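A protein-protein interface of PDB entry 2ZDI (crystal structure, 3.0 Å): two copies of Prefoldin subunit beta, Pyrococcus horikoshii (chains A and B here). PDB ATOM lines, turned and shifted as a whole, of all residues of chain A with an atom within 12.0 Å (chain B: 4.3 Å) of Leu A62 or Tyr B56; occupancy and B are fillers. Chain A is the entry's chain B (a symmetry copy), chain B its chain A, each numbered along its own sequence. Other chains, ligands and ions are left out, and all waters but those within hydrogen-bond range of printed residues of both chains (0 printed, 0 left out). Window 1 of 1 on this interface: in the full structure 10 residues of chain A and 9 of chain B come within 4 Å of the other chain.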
ATOM      1  N   GLN A  54     -26.527  25.063  18.656  1.00  0.00           N
ATOM      2  CA  GLN A  54     -26.270  24.434  19.947  1.00  0.00           C
ATOM      3  C   GLN A  54     -24.862  23.869  20.008  1.00  0.00           C
ATOM      4  O   GLN A  54     -24.559  22.861  19.370  1.00  0.00           O
ATOM      5  CB  GLN A  54     -27.281  23.323  20.218  1.00  0.00           C
ATOM      6  CG  GLN A  54     -28.697  23.812  20.439  1.00  0.00           C
ATOM      7  CD  GLN A  54     -29.635  22.692  20.828  1.00  0.00           C
ATOM      8  OE1 GLN A  54     -29.202  21.647  21.322  1.00  0.00           O
ATOM      9  NE2 GLN A  54     -30.929  22.898  20.609  1.00  0.00           N
ATOM     10  N   ILE A  55     -24.001  24.518  20.785  1.00  0.00           N
ATOM     11  CA  ILE A  55     -22.615  24.081  20.881  1.00  0.00           C
ATOM     12  C   ILE A  55     -22.327  23.450  22.249  1.00  0.00           C
ATOM     13  O   ILE A  55     -22.919  23.829  23.260  1.00  0.00           O
ATOM     14  CB  ILE A  55     -21.615  25.228  20.530  1.00  0.00           C
ATOM     15  CG1 ILE A  55     -21.075  25.907  21.785  1.00  0.00           C
ATOM     16  CG2 ILE A  55     -22.239  26.233  19.565  1.00  0.00           C
ATOM     17  CD1 ILE A  55     -19.746  25.347  22.233  1.00  0.00           C
ATOM     18  N   TYR A  56     -21.430  22.465  22.258  1.00  0.00           N
ATOM     19  CA  TYR A  56     -21.086  21.722  23.468  1.00  0.00           C
ATOM     20  C   TYR A  56     -19.615  21.895  23.839  1.00  0.00           C
ATOM     21  O   TYR A  56     -18.721  21.599  23.050  1.00  0.00           O
ATOM     22  CB  TYR A  56     -21.442  20.235  23.310  1.00  0.00           C
ATOM     23  CG  TYR A  56     -22.935  19.988  23.286  1.00  0.00           C
ATOM     24  CD1 TYR A  56     -23.625  19.677  24.449  1.00  0.00           C
ATOM     25  CD2 TYR A  56     -23.660  20.095  22.106  1.00  0.00           C
ATOM     26  CE1 TYR A  56     -24.995  19.466  24.437  1.00  0.00           C
ATOM     27  CE2 TYR A  56     -25.031  19.885  22.084  1.00  0.00           C
ATOM     28  CZ  TYR A  56     -25.694  19.572  23.252  1.00  0.00           C
ATOM     29  OH  TYR A  56     -27.058  19.364  23.238  1.00  0.00           O
ATOM     30  N   LYS A  57     -19.376  22.395  25.044  1.00  0.00           N
ATOM     31  CA  LYS A  57     -18.020  22.601  25.525  1.00  0.00           C
ATOM     32  C   LYS A  57     -17.613  21.487  26.480  1.00  0.00           C
ATOM     33  O   LYS A  57     -18.455  20.881  27.139  1.00  0.00           O
ATOM     34  CB  LYS A  57     -17.890  23.959  26.220  1.00  0.00           C
ATOM     35  CG  LYS A  57     -16.510  24.204  26.796  1.00  0.00           C
ATOM     36  CD  LYS A  57     -16.463  25.419  27.691  1.00  0.00           C
ATOM     37  CE  LYS A  57     -15.057  25.594  28.230  1.00  0.00           C
ATOM     38  NZ  LYS A  57     -14.847  26.922  28.853  1.00  0.00           N
ATOM     39  N   THR A  58     -16.314  21.222  26.542  1.00  0.00           N
ATOM     40  CA  THR A  58     -15.777  20.215  27.444  1.00  0.00           C
ATOM     41  C   THR A  58     -15.083  20.884  28.622  1.00  0.00           C
ATOM     42  O   THR A  58     -14.102  21.606  28.450  1.00  0.00           O
ATOM     43  CB  THR A  58     -14.772  19.293  26.732  1.00  0.00           C
ATOM     44  OG1 THR A  58     -15.270  18.949  25.430  1.00  0.00           O
ATOM     45  CG2 THR A  58     -14.545  18.025  27.548  1.00  0.00           C
ATOM     46  N   VAL A  59     -15.603  20.643  29.819  1.00  0.00           N
ATOM     47  CA  VAL A  59     -15.025  21.198  31.033  1.00  0.00           C
ATOM     48  C   VAL A  59     -14.287  20.101  31.796  1.00  0.00           C
ATOM     49  O   VAL A  59     -14.829  19.498  32.722  1.00  0.00           O
ATOM     50  CB  VAL A  59     -16.112  21.834  31.922  1.00  0.00           C
ATOM     51  CG1 VAL A  59     -15.483  22.618  33.064  1.00  0.00           C
ATOM     52  CG2 VAL A  59     -17.013  22.734  31.087  1.00  0.00           C
ATOM     53  N   GLY A  60     -13.046  19.845  31.393  1.00  0.00           N
ATOM     54  CA  GLY A  60     -12.262  18.768  31.966  1.00  0.00           C
ATOM     55  C   GLY A  60     -12.876  17.413  31.673  1.00  0.00           C
ATOM     56  O   GLY A  60     -12.844  16.933  30.540  1.00  0.00           O
ATOM     57  N   THR A  61     -13.441  16.797  32.704  1.00  0.00           N
ATOM     58  CA  THR A  61     -14.087  15.499  32.572  1.00  0.00           C
ATOM     59  C   THR A  61     -15.519  15.626  32.041  1.00  0.00           C
ATOM     60  O   THR A  61     -16.076  14.679  31.490  1.00  0.00           O
ATOM     61  CB  THR A  61     -14.098  14.759  33.925  1.00  0.00           C
ATOM     62  OG1 THR A  61     -15.263  13.931  34.013  1.00  0.00           O
ATOM     63  CG2 THR A  61     -14.116  15.759  35.083  1.00  0.00           C
ATOM     64  N   LEU A  62     -16.104  16.809  32.196  1.00  0.00           N
ATOM     65  CA  LEU A  62     -17.508  17.015  31.863  1.00  0.00           C
ATOM     66  C   LEU A  62     -17.727  17.641  30.494  1.00  0.00           C
ATOM     67  O   LEU A  62     -16.784  18.069  29.832  1.00  0.00           O
ATOM     68  CB  LEU A  62     -18.170  17.892  32.922  1.00  0.00           C
ATOM     69  CG  LEU A  62     -18.090  17.352  34.343  1.00  0.00           C
ATOM     70  CD1 LEU A  62     -18.516  18.419  35.331  1.00  0.00           C
ATOM     71  CD2 LEU A  62     -18.952  16.110  34.473  1.00  0.00           C
ATOM     72  N   ILE A  63     -18.991  17.684  30.087  1.00  0.00           N
ATOM     73  CA  ILE A  63     -19.397  18.341  28.853  1.00  0.00           C
ATOM     74  C   ILE A  63     -20.620  19.199  29.136  1.00  0.00           C
ATOM     75  O   ILE A  63     -21.673  18.688  29.523  1.00  0.00           O
ATOM     76  CB  ILE A  63     -19.734  17.327  27.740  1.00  0.00           C
ATOM     77  CG1 ILE A  63     -18.456  16.739  27.145  1.00  0.00           C
ATOM     78  CG2 ILE A  63     -20.545  17.984  26.641  1.00  0.00           C
ATOM     79  CD1 ILE A  63     -18.708  15.830  25.965  1.00  0.00           C
ATOM     80  N   VAL A  64     -20.475  20.508  28.957  1.00  0.00           N
ATOM     81  CA  VAL A  64     -21.582  21.425  29.182  1.00  0.00           C
ATOM     82  C   VAL A  64     -22.047  22.043  27.874  1.00  0.00           C
ATOM     83  O   VAL A  64     -21.244  22.392  27.012  1.00  0.00           O
ATOM     84  CB  VAL A  64     -21.219  22.535  30.182  1.00  0.00           C
ATOM     85  CG1 VAL A  64     -20.380  21.966  31.305  1.00  0.00           C
ATOM     86  CG2 VAL A  64     -20.480  23.664  29.486  1.00  0.00           C
ATOM     87  N   LYS A  65     -23.359  22.156  27.732  1.00  0.00           N
ATOM     88  CA  LYS A  65     -23.957  22.761  26.557  1.00  0.00           C
ATOM     89  C   LYS A  65     -23.919  24.270  26.713  1.00  0.00           C
ATOM     90  O   LYS A  65     -24.718  24.839  27.452  1.00  0.00           O
ATOM     91  CB  LYS A  65     -25.400  22.277  26.406  1.00  0.00           C
ATOM     92  CG  LYS A  65     -26.132  22.789  25.180  1.00  0.00           C
ATOM     93  CD  LYS A  65     -27.528  22.195  25.127  1.00  0.00           C
ATOM     94  CE  LYS A  65     -28.379  22.840  24.055  1.00  0.00           C
ATOM     95  NZ  LYS A  65     -29.773  22.311  24.087  1.00  0.00           N
ATOM     96  N   THR A  66     -22.973  24.913  26.036  1.00  0.00           N
ATOM     97  CA  THR A  66     -22.880  26.371  26.053  1.00  0.00           C
ATOM     98  C   THR A  66     -23.466  26.938  24.757  1.00  0.00           C
ATOM     99  O   THR A  66     -24.133  26.221  24.005  1.00  0.00           O
ATOM    100  CB  THR A  66     -21.422  26.864  26.310  1.00  0.00           C
ATOM    101  OG1 THR A  66     -21.417  28.266  26.606  1.00  0.00           O
ATOM    102  CG2 THR A  66     -20.528  26.602  25.116  1.00  0.00           C
ATOM    103  N   GLU A  74     -15.210  33.108  24.851  1.00  0.00           N
ATOM    104  CA  GLU A  74     -14.212  32.251  25.475  1.00  0.00           C
ATOM    105  C   GLU A  74     -13.066  31.972  24.515  1.00  0.00           C
ATOM    106  O   GLU A  74     -11.895  32.025  24.894  1.00  0.00           O
ATOM    107  CB  GLU A  74     -14.854  30.934  25.917  1.00  0.00           C
ATOM    108  CG  GLU A  74     -16.213  31.083  26.606  1.00  0.00           C
ATOM    109  CD  GLU A  74     -16.670  29.812  27.306  1.00  0.00           C
ATOM    110  OE1 GLU A  74     -16.001  29.400  28.274  1.00  0.00           O
ATOM    111  OE2 GLU A  74     -17.704  29.233  26.898  1.00  0.00           O
ATOM    112  N   ILE B  46     -17.868  25.217  36.450  1.00  0.00           N
ATOM    113  CA  ILE B  46     -19.230  24.703  36.547  1.00  0.00           C
ATOM    114  C   ILE B  46     -20.048  25.427  37.617  1.00  0.00           C
ATOM    115  O   ILE B  46     -21.267  25.552  37.499  1.00  0.00           O
ATOM    116  CB  ILE B  46     -19.256  23.185  36.810  1.00  0.00           C
ATOM    117  CG1 ILE B  46     -20.698  22.677  36.829  1.00  0.00           C
ATOM    118  CG2 ILE B  46     -18.569  22.857  38.121  1.00  0.00           C
ATOM    119  CD1 ILE B  46     -20.832  21.256  37.301  1.00  0.00           C
ATOM    120  N   ILE B  55     -25.706  19.401  31.465  1.00  0.00           N
ATOM    121  CA  ILE B  55     -24.357  18.869  31.598  1.00  0.00           C
ATOM    122  C   ILE B  55     -24.352  17.361  31.407  1.00  0.00           C
ATOM    123  O   ILE B  55     -25.256  16.669  31.869  1.00  0.00           O
ATOM    124  CB  ILE B  55     -23.770  19.172  32.992  1.00  0.00           C
ATOM    125  CG1 ILE B  55     -24.018  20.632  33.376  1.00  0.00           C
ATOM    126  CG2 ILE B  55     -22.284  18.841  33.034  1.00  0.00           C
ATOM    127  CD1 ILE B  55     -23.520  20.990  34.757  1.00  0.00           C
ATOM    128  N   TYR B  56     -23.334  16.852  30.721  1.00  0.00           N
ATOM    129  CA  TYR B  56     -23.132  15.412  30.627  1.00  0.00           C
ATOM    130  C   TYR B  56     -21.884  15.014  31.397  1.00  0.00           C
ATOM    131  O   TYR B  56     -20.812  15.584  31.212  1.00  0.00           O
ATOM    132  CB  TYR B  56     -23.031  14.948  29.172  1.00  0.00           C
ATOM    133  CG  TYR B  56     -24.302  15.133  28.377  1.00  0.00           C
ATOM    134  CD1 TYR B  56     -25.215  14.096  28.230  1.00  0.00           C
ATOM    135  CD2 TYR B  56     -24.590  16.348  27.767  1.00  0.00           C
ATOM    136  CE1 TYR B  56     -26.382  14.266  27.500  1.00  0.00           C
ATOM    137  CE2 TYR B  56     -25.749  16.529  27.035  1.00  0.00           C
ATOM    138  CZ  TYR B  56     -26.643  15.487  26.902  1.00  0.00           C
ATOM    139  OH  TYR B  56     -27.796  15.676  26.171  1.00  0.00           O
ATOM    140  N   LYS B  57     -22.053  14.035  32.276  1.00  0.00           N
ATOM    141  CA  LYS B  57     -20.976  13.486  33.085  1.00  0.00           C
ATOM    142  C   LYS B  57     -20.435  12.224  32.421  1.00  0.00           C
ATOM    143  O   LYS B  57     -21.197  11.435  31.863  1.00  0.00           O
ATOM    144  CB  LYS B  57     -21.513  13.179  34.486  1.00  0.00           C
ATOM    145  CG  LYS B  57     -20.929  11.954  35.173  1.00  0.00           C
ATOM    146  CD  LYS B  57     -21.911  11.434  36.221  1.00  0.00           C
ATOM    147  CE  LYS B  57     -21.233  10.549  37.258  1.00  0.00           C
ATOM    148  NZ  LYS B  57     -22.228   9.898  38.163  1.00  0.00           N
ATOM    149  N   THR B  58     -19.118  12.041  32.464  1.00  0.00           N
ATOM    150  CA  THR B  58     -18.517  10.849  31.871  1.00  0.00           C
ATOM    151  C   THR B  58     -18.332   9.718  32.883  1.00  0.00           C
ATOM    152  O   THR B  58     -17.320   9.637  33.584  1.00  0.00           O
ATOM    153  CB  THR B  58     -17.185  11.150  31.143  1.00  0.00           C
ATOM    154  OG1 THR B  58     -16.665   9.938  30.581  1.00  0.00           O
ATOM    155  CG2 THR B  58     -16.165  11.744  32.096  1.00  0.00           C
ATOM    156  N   ILE B  63     -21.469   8.375  28.624  1.00  0.00           N
ATOM    157  CA  ILE B  63     -21.563   9.821  28.783  1.00  0.00           C
ATOM    158  C   ILE B  63     -23.012  10.160  29.084  1.00  0.00           C
ATOM    159  O   ILE B  63     -23.812  10.384  28.176  1.00  0.00           O
ATOM    160  CB  ILE B  63     -21.119  10.573  27.519  1.00  0.00           C
ATOM    161  CG1 ILE B  63     -19.661  10.244  27.186  1.00  0.00           C
ATOM    162  CG2 ILE B  63     -21.309  12.076  27.704  1.00  0.00           C
ATOM    163  CD1 ILE B  63     -19.271  10.563  25.754  1.00  0.00           C
ATOM    164  N   VAL B  64     -23.344  10.177  30.368  1.00  0.00           N
ATOM    165  CA  VAL B  64     -24.723  10.351  30.802  1.00  0.00           C
ATOM    166  C   VAL B  64     -24.988  11.790  31.221  1.00  0.00           C
ATOM    167  O   VAL B  64     -24.086  12.480  31.688  1.00  0.00           O
ATOM    168  CB  VAL B  64     -25.046   9.410  31.978  1.00  0.00           C
ATOM    169  CG1 VAL B  64     -25.128   7.974  31.497  1.00  0.00           C
ATOM    170  CG2 VAL B  64     -23.992   9.545  33.066  1.00  0.00           C
ATOM    171  N   LYS B  65     -26.222  12.246  31.049  1.00  0.00           N
ATOM    172  CA  LYS B  65     -26.570  13.588  31.487  1.00  0.00           C
ATOM    173  C   LYS B  65     -26.764  13.633  32.998  1.00  0.00           C
ATOM    174  O   LYS B  65     -27.362  12.735  33.592  1.00  0.00           O
ATOM    175  CB  LYS B  65     -27.804  14.121  30.754  1.00  0.00           C
ATOM    176  CG  LYS B  65     -28.147  15.557  31.129  1.00  0.00           C
ATOM    177  CD  LYS B  65     -28.512  16.393  29.917  1.00  0.00           C
ATOM    178  CE  LYS B  65     -29.893  16.064  29.400  1.00  0.00           C
ATOM    179  NZ  LYS B  65     -30.199  16.828  28.163  1.00  0.00           N
ATOM    180  N   LEU B  75     -17.869  16.616  42.089  1.00  0.00           N
ATOM    181  CA  LEU B  75     -16.653  17.292  41.671  1.00  0.00           C
ATOM    182  C   LEU B  75     -15.840  17.725  42.883  1.00  0.00           C
ATOM    183  O   LEU B  75     -14.611  17.777  42.832  1.00  0.00           O
ATOM    184  CB  LEU B  75     -16.999  18.498  40.798  1.00  0.00           C
ATOM    185  CG  LEU B  75     -16.233  18.598  39.480  1.00  0.00           C
ATOM    186  CD1 LEU B  75     -16.756  19.763  38.661  1.00  0.00           C
ATOM    187  CD2 LEU B  75     -14.734  18.724  39.716  1.00  0.00           C
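Printed residues of chain B within 4 Å of Tyr A56: Tyr B56 (3.99 Å).
Thr A58 touches none of the printed residues of chain B.
Of the printed residues of chain B, Thr A61 touches Thr B58 (3.0 Å).
Of the printed residues of chain B, Leu A62 touches Tyr B56, Lys B57 and Leu B75.
Printed residues of chain B within 4 Å of Ile A63: Ile B55 and Tyr B56.
No residue of chain A comes within 4 Å of Ile B46.
Printed residues of chain A within 4 Å of Tyr B56: Tyr A56 (3.99 Å), Leu A62 (3.7 Å) and Ile A63 (2.8 Å).
Of the printed residues of chain A, Lys B57 touches Leu A62.
Thr B58 touches one residue of chain A.
No residue of chain A comes within 4 Å of Ile B63.
No residue of chain A comes within 4 Å of Val B64.
No residue of chain A comes within 4 Å of Lys B65.
Of the printed residues of chain A, Leu B75 touches Leu A62.
The nearest printed residue of chain B that does not touch Leu A62 is Ile B46 (4.2 Å).
The nearest printed residue of chain A that does not touch Tyr B56 is Thr A61 (4.8 Å).
The nearest printed residue of chain B that does not touch Ile A63 is Ile B63 (4.9 Å).
Tyr B56 touches its own counterpart, Tyr A56.
Ile A63 touches Ile B55, but with the chains exchanged Ile A55 does not touch Ile B63 (12.7 Å).
Ile A63 touches Tyr B56, but with the chains exchanged Tyr A56 does not touch Ile B63 (8.6 Å).
Positions printed for both chains: 55, 56, 57, 58, 63, 64 and 65.
Of the 7 pairs that touch across the chains among the printed residues, 1 has its exchanged pair printed and touching as well.
The backbone carbonyl oxygen (O) of Ile A63 sits at hydrogen-bond distance from the backbone NH (N) of Tyr B56, at 2.8 Å.
Printed residues of chain A that touch a printed residue of chain B: Tyr A56, Thr A61, Leu A62 and Ile A63.
Hydrophobic or aromatic side chains of chain B that line the printed part of chain A: Ile B55, Tyr B56 and Leu B75.
Among the printed residues, 7 pairs touch across the chains.
Among the printed residues, no Asp or Glu carboxylate lies within 4 Å of a Lys or Arg side-chain nitrogen of the other chain.
Among the printed residues, pairs that only touch across the chains: Thr A61 with Thr B58, Ile A63 with Ile B55, Leu A62 with Lys B57, Leu A62 with Tyr B56, Tyr A56 with Tyr B56 and Leu A62 with Leu B75.
OH of Tyr B56 sits at hydrogen-bond distance from NZ of Lys B65 (3.3 Å).
The backbone carbonyl oxygen (O) of Val B64 lies within hydrogen-bond range of the backbone NH (N) of Lys B57 (2.6 Å).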
